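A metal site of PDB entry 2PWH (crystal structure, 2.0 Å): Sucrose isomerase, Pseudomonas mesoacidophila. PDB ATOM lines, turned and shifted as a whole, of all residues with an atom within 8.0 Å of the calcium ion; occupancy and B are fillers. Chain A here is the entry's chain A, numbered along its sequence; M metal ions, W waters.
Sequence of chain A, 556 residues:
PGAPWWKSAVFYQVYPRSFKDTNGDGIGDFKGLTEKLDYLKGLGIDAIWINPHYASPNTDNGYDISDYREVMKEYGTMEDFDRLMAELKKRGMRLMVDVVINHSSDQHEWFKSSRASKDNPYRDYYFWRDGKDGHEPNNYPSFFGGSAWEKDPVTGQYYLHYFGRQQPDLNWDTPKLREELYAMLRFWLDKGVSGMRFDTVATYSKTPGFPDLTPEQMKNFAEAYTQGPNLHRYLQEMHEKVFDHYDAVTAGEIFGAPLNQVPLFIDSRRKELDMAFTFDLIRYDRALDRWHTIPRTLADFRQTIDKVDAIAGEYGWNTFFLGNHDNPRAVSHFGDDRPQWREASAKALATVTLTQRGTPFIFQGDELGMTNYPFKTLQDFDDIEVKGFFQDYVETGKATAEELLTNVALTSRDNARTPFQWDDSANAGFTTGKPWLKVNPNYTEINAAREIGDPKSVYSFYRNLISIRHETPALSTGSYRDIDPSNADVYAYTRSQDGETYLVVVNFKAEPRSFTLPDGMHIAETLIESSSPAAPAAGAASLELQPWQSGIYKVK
OD2 of Asp 29 is bound to the calcium ion (2.3 Å). The backbone carbonyl oxygen (O) of Ile 27 is bound to the calcium ion, at 2.3 Å. The calcium ion is bound by OD1 of Asn 23. OD1 of Asp 21 is bound to the calcium ion. Water W1 binds the calcium ion (2.4 Å). The calcium ion is bound by the side-chain carboxylate (OD1) of Asp 25, at 2.6 Å. The calcium ion is bound by water W2.
Of the 21 residues printed, 5 come within 4 Å of the calcium ion.
OD1 of Asp 29 sits at hydrogen-bond distance from N of Gly 32 (2.9 Å). OD2 of Asp 21 lies close to N of Gly 24 (3.3 Å). OG1 of Thr 431 sits at hydrogen-bond distance from OD2 of Asp 21, 2.8 Å away. OD1 of Asp 29 lies within hydrogen-bond range of OG1 of Thr 22 (2.7 Å). The backbone NH (N) of Asp 21 lies within hydrogen-bond range of the backbone carbonyl oxygen (O) of Phe 430 (3.1 Å). The backbone NH (N) of Gly 26 lies within hydrogen-bond range of the side-chain carboxylate (OD2) of Asp 21 (2.8 Å). N of Asp 29 lies within hydrogen-bond range of O of Lys 20, 3.1 Å away.
Water W1 lies within hydrogen-bond range of the side-chain amide nitrogen of Asn 23 (3.2 Å) and the backbone carbonyl oxygen of Glu 74 (3.2 Å). Water W2 bridges OD2 of Asp 25 (2.5 Å) and O of Glu 74 (2.6 Å).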
ATOM      1  N   PRO A  16      -4.046  20.436 -11.741  1.00  0.00           N
ATOM      2  CA  PRO A  16      -3.421  19.161 -11.381  1.00  0.00           C
ATOM      3  C   PRO A  16      -2.255  19.240 -10.408  1.00  0.00           C
ATOM      4  O   PRO A  16      -2.144  18.421  -9.492  1.00  0.00           O
ATOM      5  CB  PRO A  16      -2.997  18.589 -12.731  1.00  0.00           C
ATOM      6  CG  PRO A  16      -4.044  19.106 -13.649  1.00  0.00           C
ATOM      7  CD  PRO A  16      -4.170  20.548 -13.197  1.00  0.00           C
ATOM      8  N   ARG A  17      -1.385  20.210 -10.617  1.00  0.00           N
ATOM      9  CA  ARG A  17      -0.207  20.404  -9.770  1.00  0.00           C
ATOM     10  C   ARG A  17      -0.561  20.557  -8.289  1.00  0.00           C
ATOM     11  O   ARG A  17       0.212  20.163  -7.407  1.00  0.00           O
ATOM     12  CB  ARG A  17       0.572  21.632 -10.246  1.00  0.00           C
ATOM     13  CG  ARG A  17       1.950  21.775  -9.637  1.00  0.00           C
ATOM     14  CD  ARG A  17       2.665  23.037 -10.108  1.00  0.00           C
ATOM     15  NE  ARG A  17       3.996  23.143  -9.520  1.00  0.00           N
ATOM     16  CZ  ARG A  17       5.054  22.434  -9.915  1.00  0.00           C
ATOM     17  NH1 ARG A  17       4.956  21.561 -10.905  1.00  0.00           N
ATOM     18  NH2 ARG A  17       6.226  22.589  -9.294  1.00  0.00           N
ATOM     19  N   LYS A  20      -4.354  16.746  -6.197  1.00  0.00           N
ATOM     20  CA  LYS A  20      -4.154  15.551  -5.374  1.00  0.00           C
ATOM     21  C   LYS A  20      -2.919  14.737  -5.763  1.00  0.00           C
ATOM     22  O   LYS A  20      -2.833  14.199  -6.873  1.00  0.00           O
ATOM     23  CB  LYS A  20      -5.398  14.660  -5.450  1.00  0.00           C
ATOM     24  CG  LYS A  20      -5.303  13.378  -4.635  1.00  0.00           C
ATOM     25  CD  LYS A  20      -5.120  13.666  -3.147  1.00  0.00           C
ATOM     26  CE  LYS A  20      -5.160  12.389  -2.321  1.00  0.00           C
ATOM     27  NZ  LYS A  20      -4.106  11.425  -2.724  1.00  0.00           N
ATOM     28  N   ASP A  21      -1.960  14.633  -4.838  1.00  0.00           N
ATOM     29  CA  ASP A  21      -0.735  13.878  -5.049  1.00  0.00           C
ATOM     30  C   ASP A  21      -0.942  12.441  -4.566  1.00  0.00           C
ATOM     31  O   ASP A  21      -1.559  12.208  -3.529  1.00  0.00           O
ATOM     32  CB  ASP A  21       0.427  14.530  -4.282  1.00  0.00           C
ATOM     33  CG  ASP A  21       1.727  13.737  -4.371  1.00  0.00           C
ATOM     34  OD1 ASP A  21       1.847  12.866  -5.260  1.00  0.00           O
ATOM     35  OD2 ASP A  21       2.628  13.994  -3.548  1.00  0.00           O
ATOM     36  N   THR A  22      -0.433  11.464  -5.318  1.00  0.00           N
ATOM     37  CA  THR A  22      -0.593  10.058  -4.944  1.00  0.00           C
ATOM     38  C   THR A  22       0.714   9.271  -4.831  1.00  0.00           C
ATOM     39  O   THR A  22       0.681   8.059  -4.618  1.00  0.00           O
ATOM     40  CB  THR A  22      -1.499   9.300  -5.953  1.00  0.00           C
ATOM     41  OG1 THR A  22      -0.928   9.393  -7.261  1.00  0.00           O
ATOM     42  CG2 THR A  22      -2.907   9.883  -5.956  1.00  0.00           C
ATOM     43  N   ASN A  23       1.851   9.943  -4.961  1.00  0.00           N
ATOM     44  CA  ASN A  23       3.124   9.234  -4.872  1.00  0.00           C
ATOM     45  C   ASN A  23       4.121   9.960  -3.959  1.00  0.00           C
ATOM     46  O   ASN A  23       5.322   9.721  -4.031  1.00  0.00           O
ATOM     47  CB  ASN A  23       3.709   9.017  -6.271  1.00  0.00           C
ATOM     48  CG  ASN A  23       4.274  10.277  -6.877  1.00  0.00           C
ATOM     49  OD1 ASN A  23       3.740  11.372  -6.673  1.00  0.00           O
ATOM     50  ND2 ASN A  23       5.356  10.141  -7.634  1.00  0.00           N
ATOM     51  N   GLY A  24       3.596  10.855  -3.139  1.00  0.00           N
ATOM     52  CA  GLY A  24       4.411  11.592  -2.192  1.00  0.00           C
ATOM     53  C   GLY A  24       5.501  12.543  -2.635  1.00  0.00           C
ATOM     54  O   GLY A  24       6.338  12.924  -1.818  1.00  0.00           O
ATOM     55  N   ASP A  25       5.529  12.941  -3.904  1.00  0.00           N
ATOM     56  CA  ASP A  25       6.577  13.861  -4.332  1.00  0.00           C
ATOM     57  C   ASP A  25       6.174  15.320  -4.096  1.00  0.00           C
ATOM     58  O   ASP A  25       6.927  16.236  -4.401  1.00  0.00           O
ATOM     59  CB  ASP A  25       6.931  13.641  -5.809  1.00  0.00           C
ATOM     60  CG  ASP A  25       5.799  13.991  -6.753  1.00  0.00           C
ATOM     61  OD1 ASP A  25       4.677  14.299  -6.296  1.00  0.00           O
ATOM     62  OD2 ASP A  25       6.029  13.949  -7.972  1.00  0.00           O
ATOM     63  N   GLY A  26       4.974  15.510  -3.544  1.00  0.00           N
ATOM     64  CA  GLY A  26       4.500  16.848  -3.249  1.00  0.00           C
ATOM     65  C   GLY A  26       3.792  17.547  -4.395  1.00  0.00           C
ATOM     66  O   GLY A  26       3.405  18.713  -4.265  1.00  0.00           O
ATOM     67  N   ILE A  27       3.614  16.862  -5.519  1.00  0.00           N
ATOM     68  CA  ILE A  27       2.948  17.459  -6.670  1.00  0.00           C
ATOM     69  C   ILE A  27       1.730  16.632  -7.095  1.00  0.00           C
ATOM     70  O   ILE A  27       1.798  15.418  -7.192  1.00  0.00           O
ATOM     71  CB  ILE A  27       3.923  17.577  -7.858  1.00  0.00           C
ATOM     72  CG1 ILE A  27       5.091  18.486  -7.466  1.00  0.00           C
ATOM     73  CG2 ILE A  27       3.204  18.129  -9.067  1.00  0.00           C
ATOM     74  CD1 ILE A  27       6.250  18.486  -8.455  1.00  0.00           C
ATOM     75  N   GLY A  28       0.615  17.310  -7.357  1.00  0.00           N
ATOM     76  CA  GLY A  28      -0.585  16.626  -7.779  1.00  0.00           C
ATOM     77  C   GLY A  28      -0.340  15.876  -9.079  1.00  0.00           C
ATOM     78  O   GLY A  28       0.512  16.286  -9.864  1.00  0.00           O
ATOM     79  N   ASP A  29      -1.083  14.803  -9.302  1.00  0.00           N
ATOM     80  CA  ASP A  29      -0.908  14.000 -10.506  1.00  0.00           C
ATOM     81  C   ASP A  29      -2.247  13.502 -11.064  1.00  0.00           C
ATOM     82  O   ASP A  29      -3.310  13.750 -10.470  1.00  0.00           O
ATOM     83  CB  ASP A  29       0.017  12.829 -10.179  1.00  0.00           C
ATOM     84  CG  ASP A  29      -0.284  12.208  -8.819  1.00  0.00           C
ATOM     85  OD1 ASP A  29      -1.408  11.678  -8.633  1.00  0.00           O
ATOM     86  OD2 ASP A  29       0.598  12.262  -7.946  1.00  0.00           O
ATOM     87  N   PHE A  30      -2.202  12.800 -12.191  1.00  0.00           N
ATOM     88  CA  PHE A  30      -3.412  12.270 -12.807  1.00  0.00           C
ATOM     89  C   PHE A  30      -4.137  11.249 -11.952  1.00  0.00           C
ATOM     90  O   PHE A  30      -5.358  11.286 -11.829  1.00  0.00           O
ATOM     91  CB  PHE A  30      -3.111  11.683 -14.179  1.00  0.00           C
ATOM     92  CG  PHE A  30      -2.973  12.706 -15.258  1.00  0.00           C
ATOM     93  CD1 PHE A  30      -3.887  13.766 -15.349  1.00  0.00           C
ATOM     94  CD2 PHE A  30      -1.950  12.630 -16.193  1.00  0.00           C
ATOM     95  CE1 PHE A  30      -3.777  14.722 -16.350  1.00  0.00           C
ATOM     96  CE2 PHE A  30      -1.832  13.583 -17.190  1.00  0.00           C
ATOM     97  CZ  PHE A  30      -2.743  14.633 -17.270  1.00  0.00           C
ATOM     98  N   LYS A  31      -3.390  10.305 -11.371  1.00  0.00           N
ATOM     99  CA  LYS A  31      -4.024   9.302 -10.520  1.00  0.00           C
ATOM    100  C   LYS A  31      -4.796   9.989  -9.396  1.00  0.00           C
ATOM    101  O   LYS A  31      -5.877   9.538  -9.009  1.00  0.00           O
ATOM    102  CB  LYS A  31      -2.970   8.356  -9.916  1.00  0.00           C
ATOM    103  CG  LYS A  31      -2.307   7.444 -10.928  1.00  0.00           C
ATOM    104  CD  LYS A  31      -1.321   6.501 -10.265  1.00  0.00           C
ATOM    105  CE  LYS A  31      -0.640   5.602 -11.281  1.00  0.00           C
ATOM    106  NZ  LYS A  31       0.363   4.697 -10.648  1.00  0.00           N
ATOM    107  N   GLY A  32      -4.228  11.084  -8.890  1.00  0.00           N
ATOM    108  CA  GLY A  32      -4.883  11.822  -7.819  1.00  0.00           C
ATOM    109  C   GLY A  32      -6.225  12.390  -8.267  1.00  0.00           C
ATOM    110  O   GLY A  32      -7.224  12.283  -7.559  1.00  0.00           O
ATOM    111  N   LYS A  73       5.737  14.588 -17.107  1.00  0.00           N
ATOM    112  CA  LYS A  73       6.282  13.524 -16.274  1.00  0.00           C
ATOM    113  C   LYS A  73       5.678  13.508 -14.865  1.00  0.00           C
ATOM    114  O   LYS A  73       5.284  12.445 -14.370  1.00  0.00           O
ATOM    115  CB  LYS A  73       7.804  13.664 -16.179  1.00  0.00           C
ATOM    116  N   GLU A  74       5.591  14.668 -14.235  1.00  0.00           N
ATOM    117  CA  GLU A  74       5.030  14.786 -12.892  1.00  0.00           C
ATOM    118  C   GLU A  74       3.589  14.264 -12.750  1.00  0.00           C
ATOM    119  O   GLU A  74       3.229  13.693 -11.723  1.00  0.00           O
ATOM    120  CB  GLU A  74       5.064  16.242 -12.420  1.00  0.00           C
ATOM    121  CG  GLU A  74       6.436  16.812 -12.093  1.00  0.00           C
ATOM    122  CD  GLU A  74       7.329  16.973 -13.301  1.00  0.00           C
ATOM    123  OE1 GLU A  74       6.809  17.295 -14.400  1.00  0.00           O
ATOM    124  OE2 GLU A  74       8.554  16.801 -13.167  1.00  0.00           O
ATOM    125  N   TYR A  75       2.764  14.454 -13.780  1.00  0.00           N
ATOM    126  CA  TYR A  75       1.369  14.014 -13.696  1.00  0.00           C
ATOM    127  C   TYR A  75       1.133  12.542 -14.007  1.00  0.00           C
ATOM    128  O   TYR A  75       0.093  11.991 -13.643  1.00  0.00           O
ATOM    129  CB  TYR A  75       0.479  14.883 -14.593  1.00  0.00           C
ATOM    130  CG  TYR A  75       0.525  16.364 -14.276  1.00  0.00           C
ATOM    131  CD1 TYR A  75       1.087  16.822 -13.074  1.00  0.00           C
ATOM    132  CD2 TYR A  75       0.011  17.314 -15.163  1.00  0.00           C
ATOM    133  CE1 TYR A  75       1.149  18.188 -12.787  1.00  0.00           C
ATOM    134  CE2 TYR A  75       0.073  18.680 -14.876  1.00  0.00           C
ATOM    135  CZ  TYR A  75       0.645  19.109 -13.687  1.00  0.00           C
ATOM    136  OH  TYR A  75       0.747  20.445 -13.403  1.00  0.00           O
ATOM    137  N   GLY A  76       2.094  11.909 -14.675  1.00  0.00           N
ATOM    138  CA  GLY A  76       1.932  10.505 -14.997  1.00  0.00           C
ATOM    139  C   GLY A  76       2.331  10.178 -16.421  1.00  0.00           C
ATOM    140  O   GLY A  76       3.193  10.848 -16.996  1.00  0.00           O
ATOM    141  N   PHE A 430      -3.452  16.371   1.040  1.00  0.00           N
ATOM    142  CA  PHE A 430      -3.029  16.588  -0.338  1.00  0.00           C
ATOM    143  C   PHE A 430      -1.875  15.663  -0.706  1.00  0.00           C
ATOM    144  O   PHE A 430      -1.848  15.100  -1.811  1.00  0.00           O
ATOM    145  CB  PHE A 430      -2.582  18.035  -0.544  1.00  0.00           C
ATOM    146  CG  PHE A 430      -1.790  18.248  -1.799  1.00  0.00           C
ATOM    147  CD1 PHE A 430      -2.388  18.115  -3.052  1.00  0.00           C
ATOM    148  CD2 PHE A 430      -0.431  18.537  -1.732  1.00  0.00           C
ATOM    149  CE1 PHE A 430      -1.640  18.263  -4.222  1.00  0.00           C
ATOM    150  CE2 PHE A 430       0.332  18.686  -2.885  1.00  0.00           C
ATOM    151  CZ  PHE A 430      -0.277  18.542  -4.146  1.00  0.00           C
ATOM    152  N   THR A 431      -0.920  15.502   0.213  1.00  0.00           N
ATOM    153  CA  THR A 431       0.250  14.665  -0.051  1.00  0.00           C
ATOM    154  C   THR A 431       0.771  14.018   1.226  1.00  0.00           C
ATOM    155  O   THR A 431       0.472  14.476   2.332  1.00  0.00           O
ATOM    156  CB  THR A 431       1.379  15.517  -0.682  1.00  0.00           C
ATOM    157  OG1 THR A 431       2.548  14.706  -0.888  1.00  0.00           O
ATOM    158  CG2 THR A 431       1.749  16.682   0.237  1.00  0.00           C
HETATM  159 CA    CA M   1       2.607  13.270  -7.454  1.00  0.00          CA
HETATM  160  O   HOH W   1       3.019  11.661  -9.232  1.00  0.00           O
HETATM  161  O   HOH W   2       4.003  14.494  -9.332  1.00  0.00           O
